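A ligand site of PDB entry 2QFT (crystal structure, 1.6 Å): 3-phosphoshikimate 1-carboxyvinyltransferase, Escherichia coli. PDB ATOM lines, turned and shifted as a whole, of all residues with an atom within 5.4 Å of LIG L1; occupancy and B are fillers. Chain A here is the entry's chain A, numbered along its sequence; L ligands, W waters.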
ATOM      1  N   LYS A  22     -14.736  31.854 -24.437  1.00  0.00           N
ATOM      2  CA  LYS A  22     -15.274  31.891 -23.079  1.00  0.00           C
ATOM      3  C   LYS A  22     -14.443  32.871 -22.218  1.00  0.00           C
ATOM      4  O   LYS A  22     -15.005  33.673 -21.474  1.00  0.00           O
ATOM      5  CB  LYS A  22     -15.239  30.474 -22.472  1.00  0.00           C
ATOM      6  CG  LYS A  22     -15.632  30.404 -20.980  1.00  0.00           C
ATOM      7  CD  LYS A  22     -14.470  29.988 -20.057  1.00  0.00           C
ATOM      8  CE  LYS A  22     -14.182  28.490 -20.195  1.00  0.00           C
ATOM      9  NZ  LYS A  22     -12.907  28.102 -19.531  1.00  0.00           N
ATOM     10  N   SER A  23     -13.123  32.770 -22.331  1.00  0.00           N
ATOM     11  CA  SER A  23     -12.223  33.618 -21.556  1.00  0.00           C
ATOM     12  C   SER A  23     -12.425  35.110 -21.843  1.00  0.00           C
ATOM     13  O   SER A  23     -12.491  35.939 -20.914  1.00  0.00           O
ATOM     14  CB  SER A  23     -10.772  33.249 -21.865  1.00  0.00           C
ATOM     15  OG  SER A  23     -10.478  31.958 -21.352  1.00  0.00           O
ATOM     16  N   ARG A  27     -14.589  38.112 -19.281  1.00  0.00           N
ATOM     17  CA  ARG A  27     -13.862  39.307 -18.870  1.00  0.00           C
ATOM     18  C   ARG A  27     -14.594  40.529 -19.441  1.00  0.00           C
ATOM     19  O   ARG A  27     -14.820  41.518 -18.738  1.00  0.00           O
ATOM     20  CB  ARG A  27     -12.446  39.295 -19.420  1.00  0.00           C
ATOM     21  CG  ARG A  27     -11.474  38.386 -18.671  1.00  0.00           C
ATOM     22  CD  ARG A  27     -10.224  38.239 -19.523  1.00  0.00           C
ATOM     23  NE  ARG A  27      -9.138  37.486 -18.904  1.00  0.00           N
ATOM     24  CZ  ARG A  27      -9.125  36.160 -18.731  1.00  0.00           C
ATOM     25  NH1 ARG A  27      -8.068  35.578 -18.167  1.00  0.00           N
ATOM     26  NH2 ARG A  27     -10.187  35.430 -19.099  1.00  0.00           N
ATOM     27  N   THR A  97     -14.009  31.177 -14.361  1.00  0.00           N
ATOM     28  CA  THR A  97     -13.789  32.540 -14.831  1.00  0.00           C
ATOM     29  C   THR A  97     -14.766  33.500 -14.179  1.00  0.00           C
ATOM     30  O   THR A  97     -14.435  34.672 -14.008  1.00  0.00           O
ATOM     31  CB  THR A  97     -13.876  32.664 -16.379  1.00  0.00           C
ATOM     32  OG1 THR A  97     -15.149  32.180 -16.835  1.00  0.00           O
ATOM     33  CG2 THR A  97     -12.758  31.886 -17.040  1.00  0.00           C
ATOM     34  N   ARG A 100     -13.938  33.168  -9.795  1.00  0.00           N
ATOM     35  CA  ARG A 100     -12.748  33.866  -9.342  1.00  0.00           C
ATOM     36  C   ARG A 100     -12.844  35.367  -9.581  1.00  0.00           C
ATOM     37  O   ARG A 100     -12.618  36.157  -8.654  1.00  0.00           O
ATOM     38  CB  ARG A 100     -11.486  33.290 -10.001  1.00  0.00           C
ATOM     39  CG  ARG A 100     -10.946  31.975  -9.362  1.00  0.00           C
ATOM     40  CD  ARG A 100     -11.908  30.780  -9.542  1.00  0.00           C
ATOM     41  NE  ARG A 100     -11.378  29.523  -8.974  1.00  0.00           N
ATOM     42  CZ  ARG A 100     -10.666  28.630  -9.647  1.00  0.00           C
ATOM     43  NH1 ARG A 100     -10.235  27.522  -9.042  1.00  0.00           N
ATOM     44  NH2 ARG A 100     -10.380  28.834 -10.940  1.00  0.00           N
ATOM     45  N   VAL A 168      -1.135  27.616  -8.756  1.00  0.00           N
ATOM     46  CA  VAL A 168      -2.244  26.697  -9.022  1.00  0.00           C
ATOM     47  C   VAL A 168      -3.196  27.244 -10.085  1.00  0.00           C
ATOM     48  O   VAL A 168      -3.715  26.486 -10.904  1.00  0.00           O
ATOM     49  CB  VAL A 168      -2.986  26.378  -7.694  1.00  0.00           C
ATOM     50  CG1 VAL A 168      -4.251  25.569  -7.956  1.00  0.00           C
ATOM     51  CG2 VAL A 168      -2.050  25.595  -6.778  1.00  0.00           C
ATOM     52  N   SER A 169      -3.462  28.546 -10.070  1.00  0.00           N
ATOM     53  CA  SER A 169      -4.325  29.128 -11.098  1.00  0.00           C
ATOM     54  C   SER A 169      -3.928  30.558 -11.405  1.00  0.00           C
ATOM     55  O   SER A 169      -3.605  31.325 -10.501  1.00  0.00           O
ATOM     56  CB  SER A 169      -5.804  29.123 -10.663  1.00  0.00           C
ATOM     57  OG  SER A 169      -6.647  29.702 -11.669  1.00  0.00           O
ATOM     58  N   SER A 170      -3.937  30.903 -12.681  1.00  0.00           N
ATOM     59  CA  SER A 170      -3.651  32.269 -13.102  1.00  0.00           C
ATOM     60  C   SER A 170      -4.908  33.113 -12.823  1.00  0.00           C
ATOM     61  O   SER A 170      -4.851  34.343 -12.812  1.00  0.00           O
ATOM     62  CB  SER A 170      -3.321  32.341 -14.606  1.00  0.00           C
ATOM     63  OG  SER A 170      -4.455  32.044 -15.437  1.00  0.00           O
ATOM     64  N   GLN A 171      -6.045  32.451 -12.613  1.00  0.00           N
ATOM     65  CA  GLN A 171      -7.290  33.194 -12.399  1.00  0.00           C
ATOM     66  C   GLN A 171      -7.316  34.059 -11.159  1.00  0.00           C
ATOM     67  O   GLN A 171      -8.048  35.052 -11.105  1.00  0.00           O
ATOM     68  CB  GLN A 171      -8.492  32.244 -12.383  1.00  0.00           C
ATOM     69  CG  GLN A 171      -8.738  31.599 -13.743  1.00  0.00           C
ATOM     70  CD  GLN A 171     -10.018  30.831 -13.770  1.00  0.00           C
ATOM     71  OE1 GLN A 171     -10.805  30.858 -12.808  1.00  0.00           O
ATOM     72  NE2 GLN A 171     -10.268  30.130 -14.887  1.00  0.00           N
ATOM     73  N   THR A 174      -5.558  37.176 -12.265  1.00  0.00           N
ATOM     74  CA  THR A 174      -6.453  37.868 -13.178  1.00  0.00           C
ATOM     75  C   THR A 174      -7.555  38.616 -12.412  1.00  0.00           C
ATOM     76  O   THR A 174      -7.856  39.781 -12.723  1.00  0.00           O
ATOM     77  CB  THR A 174      -7.105  36.887 -14.174  1.00  0.00           C
ATOM     78  OG1 THR A 174      -6.200  36.699 -15.272  1.00  0.00           O
ATOM     79  CG2 THR A 174      -8.469  37.415 -14.702  1.00  0.00           C
ATOM     80  N   VAL A 196       1.522  29.838 -13.249  1.00  0.00           N
ATOM     81  CA  VAL A 196       1.080  28.914 -14.282  1.00  0.00           C
ATOM     82  C   VAL A 196       0.068  29.601 -15.185  1.00  0.00           C
ATOM     83  O   VAL A 196      -0.443  30.678 -14.860  1.00  0.00           O
ATOM     84  CB  VAL A 196       0.455  27.623 -13.686  1.00  0.00           C
ATOM     85  CG1 VAL A 196       1.528  26.847 -12.914  1.00  0.00           C
ATOM     86  CG2 VAL A 196      -0.761  27.967 -12.793  1.00  0.00           C
ATOM     87  N   SER A 197      -0.166  28.996 -16.350  1.00  0.00           N
ATOM     88  CA  SER A 197      -1.115  29.522 -17.308  1.00  0.00           C
ATOM     89  C   SER A 197      -0.881  30.992 -17.617  1.00  0.00           C
ATOM     90  O   SER A 197      -1.817  31.773 -17.787  1.00  0.00           O
ATOM     91  CB  SER A 197      -2.541  29.321 -16.778  1.00  0.00           C
ATOM     92  OG  SER A 197      -2.852  27.933 -16.801  1.00  0.00           O
ATOM     93  N   TYR A 200      -2.905  33.542 -19.999  1.00  0.00           N
ATOM     94  CA  TYR A 200      -4.217  34.106 -19.633  1.00  0.00           C
ATOM     95  C   TYR A 200      -4.085  35.462 -18.963  1.00  0.00           C
ATOM     96  O   TYR A 200      -5.018  36.273 -18.998  1.00  0.00           O
ATOM     97  CB  TYR A 200      -5.017  33.119 -18.768  1.00  0.00           C
ATOM     98  CG  TYR A 200      -5.490  31.946 -19.584  1.00  0.00           C
ATOM     99  CD1 TYR A 200      -4.710  30.793 -19.673  1.00  0.00           C
ATOM    100  CD2 TYR A 200      -6.704  31.982 -20.283  1.00  0.00           C
ATOM    101  CE1 TYR A 200      -5.133  29.697 -20.422  1.00  0.00           C
ATOM    102  CE2 TYR A 200      -7.129  30.893 -21.039  1.00  0.00           C
ATOM    103  CZ  TYR A 200      -6.339  29.764 -21.102  1.00  0.00           C
ATOM    104  OH  TYR A 200      -6.745  28.672 -21.835  1.00  0.00           O
ATOM    105  N   PRO A 312      -2.771  24.612 -21.188  1.00  0.00           N
ATOM    106  CA  PRO A 312      -3.372  23.500 -20.440  1.00  0.00           C
ATOM    107  C   PRO A 312      -4.701  22.917 -20.938  1.00  0.00           C
ATOM    108  O   PRO A 312      -4.923  21.710 -20.824  1.00  0.00           O
ATOM    109  CB  PRO A 312      -3.479  24.055 -19.011  1.00  0.00           C
ATOM    110  CG  PRO A 312      -3.726  25.523 -19.234  1.00  0.00           C
ATOM    111  CD  PRO A 312      -2.714  25.848 -20.371  1.00  0.00           C
ATOM    112  N   ASP A 313      -5.557  23.773 -21.477  1.00  0.00           N
ATOM    113  CA  ASP A 313      -6.869  23.313 -21.940  1.00  0.00           C
ATOM    114  C   ASP A 313      -6.775  22.607 -23.293  1.00  0.00           C
ATOM    115  O   ASP A 313      -7.223  21.459 -23.449  1.00  0.00           O
ATOM    116  CB  ASP A 313      -7.855  24.491 -22.037  1.00  0.00           C
ATOM    117  CG  ASP A 313      -8.169  25.116 -20.674  1.00  0.00           C
ATOM    118  OD1 ASP A 313      -8.882  26.137 -20.671  1.00  0.00           O
ATOM    119  OD2 ASP A 313      -7.701  24.616 -19.625  1.00  0.00           O
ATOM    120  N   ASN A 336      -2.369  21.407 -12.774  1.00  0.00           N
ATOM    121  CA  ASN A 336      -3.695  21.924 -12.496  1.00  0.00           C
ATOM    122  C   ASN A 336      -4.861  21.319 -13.263  1.00  0.00           C
ATOM    123  O   ASN A 336      -6.010  21.658 -13.047  1.00  0.00           O
ATOM    124  CB  ASN A 336      -3.701  23.481 -12.381  1.00  0.00           C
ATOM    125  CG  ASN A 336      -3.713  24.224 -13.696  1.00  0.00           C
ATOM    126  OD1 ASN A 336      -3.606  25.464 -13.685  1.00  0.00           O
ATOM    127  ND2 ASN A 336      -3.857  23.524 -14.810  1.00  0.00           N
ATOM    128  N   LYS A 340      -9.522  21.273 -12.036  1.00  0.00           N
ATOM    129  CA  LYS A 340     -10.461  21.933 -12.943  1.00  0.00           C
ATOM    130  C   LYS A 340     -11.839  21.248 -13.002  1.00  0.00           C
ATOM    131  O   LYS A 340     -12.307  20.805 -11.957  1.00  0.00           O
ATOM    132  CB  LYS A 340      -9.808  22.129 -14.320  1.00  0.00           C
ATOM    133  CG  LYS A 340      -8.765  23.278 -14.218  1.00  0.00           C
ATOM    134  CD  LYS A 340      -7.878  23.409 -15.433  1.00  0.00           C
ATOM    135  CE  LYS A 340      -7.077  24.717 -15.292  1.00  0.00           C
ATOM    136  NZ  LYS A 340      -5.995  24.817 -16.308  1.00  0.00           N
ATOM    137  N   ARG A 386     -14.629  19.147 -21.997  1.00  0.00           N
ATOM    138  CA  ARG A 386     -13.491  18.710 -22.790  1.00  0.00           C
ATOM    139  C   ARG A 386     -13.267  17.208 -22.848  1.00  0.00           C
ATOM    140  O   ARG A 386     -12.649  16.731 -23.787  1.00  0.00           O
ATOM    141  CB  ARG A 386     -12.204  19.446 -22.365  1.00  0.00           C
ATOM    142  CG  ARG A 386     -12.324  20.972 -22.567  1.00  0.00           C
ATOM    143  CD  ARG A 386     -10.948  21.692 -22.726  1.00  0.00           C
ATOM    144  NE  ARG A 386     -11.205  23.111 -22.533  1.00  0.00           N
ATOM    145  CZ  ARG A 386     -11.816  23.894 -23.414  1.00  0.00           C
ATOM    146  NH1 ARG A 386     -12.054  25.167 -23.084  1.00  0.00           N
ATOM    147  NH2 ARG A 386     -12.121  23.460 -24.637  1.00  0.00           N
HETATM  148  C1  LIG L   1      -8.811  30.810 -17.890  1.00  0.00           C
HETATM  149  C2  LIG L   1      -7.590  30.420 -17.296  1.00  0.00           C
HETATM  150  C3  LIG L   1      -7.208  28.947 -17.184  1.00  0.00           C
HETATM  151  C4  LIG L   1      -8.053  28.031 -18.107  1.00  0.00           C
HETATM  152  C5  LIG L   1      -9.552  28.379 -18.008  1.00  0.00           C
HETATM  153  C6  LIG L   1      -9.732  29.836 -18.442  1.00  0.00           C
HETATM  154  C7  LIG L   1      -9.142  32.274 -17.963  1.00  0.00           C
HETATM  155  O1  LIG L   1      -7.242  28.497 -15.799  1.00  0.00           O
HETATM  156  O2  LIG L   1      -7.766  26.657 -17.794  1.00  0.00           O
HETATM  157  O3  LIG L   1     -10.331  27.523 -18.859  1.00  0.00           O
HETATM  158  O4  LIG L   1      -8.623  33.042 -17.098  1.00  0.00           O
HETATM  159  O5  LIG L   1      -9.886  32.650 -18.876  1.00  0.00           O
HETATM  160  P1  LIG L   1      -5.918  28.290 -14.871  1.00  0.00           P
HETATM  161  O6  LIG L   1      -5.236  29.620 -14.767  1.00  0.00           O
HETATM  162  O7  LIG L   1      -5.029  27.259 -15.557  1.00  0.00           O
HETATM  163  O8  LIG L   1      -6.415  27.817 -13.546  1.00  0.00           O
HETATM  164  P1  LG2 L   2     -12.666  27.251 -15.468  1.00  0.00           P
HETATM  165  O1  LG2 L   2     -12.848  28.148 -16.637  1.00  0.00           O
HETATM  166  O2  LG2 L   2     -11.888  27.876 -14.351  1.00  0.00           O
HETATM  167  O3  LG2 L   2     -13.967  26.708 -14.994  1.00  0.00           O
HETATM  168  O4  LG2 L   2     -12.102  25.296 -20.007  1.00  0.00           O
HETATM  169  O5  LG2 L   2     -10.740  23.555 -20.072  1.00  0.00           O
HETATM  170  C1  LG2 L   2     -11.665  25.930 -15.945  1.00  0.00           C
HETATM  171  C2  LG2 L   2     -11.030  24.550 -17.973  1.00  0.00           C
HETATM  172  C3  LG2 L   2     -11.306  24.455 -19.464  1.00  0.00           C
HETATM  173  N1  LG2 L   2     -11.810  25.638 -17.362  1.00  0.00           N
HETATM  174  O   HOH W   1      -9.194  27.379 -13.203  1.00  0.00           O
HETATM  175  O   HOH W   2      -6.507  25.885 -11.788  1.00  0.00           O
HETATM  176  O   HOH W   3      -6.403  33.978 -15.696  1.00  0.00           O
HETATM  177  O   HOH W   4     -10.571  34.407 -15.399  1.00  0.00           O
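O3 of LIG L1 lies within hydrogen-bond range of N1 of LG2 L2 (2.8 Å).
NH2 of Arg 27 sits at hydrogen-bond distance from O of Ser 23, 3.0 Å away. The side-chain hydroxyl (OG) of Ser 169 sits at hydrogen-bond distance from the backbone NH (N) of Gln 171 (3.0 Å). OD2 of Asp 313 lies within salt-bridge range of NZ of Lys 340, 3.7 Å away. ND2 of Asn 336 sits close to NZ of Lys 340 (2.9 Å). The guanidinium group (NH1) of Arg 27 is in hydrogen-bond range of the backbone carbonyl oxygen (O) of Tyr 200 (3.2 Å). The side-chain amide oxygen of Asn 336 lies close to the backbone carbonyl oxygen of Val 168, 3.0 Å away. NH2 of Arg 100 is in hydrogen-bond range of OE1 of Gln 171.
Merely in contact with LIG L1: Thr 97, Gln 171 and Tyr 200. Hydrophobic or aromatic side chains that line LIG L1: Tyr 200. 12 residues have an atom within 4 Å of LIG L1: Lys 22, Ser 23, Arg 27, Thr 97, Ser 169, Ser 170, Gln 171, Ser 197, Tyr 200, Asp 313, Asn 336 and Lys 340.
The side-chain hydroxyl of Ser 197 is in hydrogen-bond range of an oxygen (O7) of LIG L1, at 2.6 Å. The backbone NH of Ser 170 is in hydrogen-bond range of an oxygen (O6) of LIG L1, 2.8 Å away. An oxygen (O6) of LIG L1 is in hydrogen-bond range of the side-chain hydroxyl (OG) of Ser 170 (2.6 Å). O5 of LIG L1 sits at hydrogen-bond distance from OG of Ser 23 (2.6 Å). The side-chain hydroxyl of Ser 169 lies within hydrogen-bond range of an oxygen (O8) of LIG L1 (2.7 Å). An oxygen (O3) of LIG L1 is in hydrogen-bond range of the side-chain carboxylate (OD1) of Asp 313, 2.7 Å away. The side-chain amino group (NZ) of Lys 22 sits at hydrogen-bond distance from an oxygen (O3) of LIG L1, 2.7 Å away. O7 of LIG L1 lies within salt-bridge range of NZ of Lys 340, at 2.7 Å. NH2 of Arg 27 lies within salt-bridge range of O5 of LIG L1 (2.8 Å). O7 of LIG L1 sits close to OD1 of Asn 336 (3.0 Å). NZ of Lys 22 lies within salt-bridge range of O1 of LG2 L2 (2.9 Å). O2 of LG2 L2 is in hydrogen-bond range of NE2 of Gln 171, 2.8 Å away. An oxygen (O2) of LG2 L2 is in salt-bridge range of the guanidinium group (NH2) of Arg 100 (3.9 Å). O5 of LG2 L2 is in salt-bridge range of NE of Arg 386 (2.5 Å).
Water W2 lies within hydrogen-bond range of an oxygen (O8) of LIG L1 (2.6 Å), the backbone carbonyl oxygen of Val 168 (3.0 Å) and the side-chain amide oxygen of Asn 336 (3.5 Å). Water W3 lies within hydrogen-bond range of OG of Ser 170 (2.8 Å), OG1 of Thr 174 (2.8 Å), O4 of LIG L1 (2.8 Å), NH1 of Arg 27 (3.4 Å) and N of Gln 171 (3.5 Å). Water W1 lies within hydrogen-bond range of an oxygen (O8) of LIG L1 (2.8 Å), the guanidinium group of Arg 100 (2.9 Å), an oxygen (O2) of LG2 L2 (3.0 Å) and the side-chain amide nitrogen of Gln 171 (3.4 Å).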
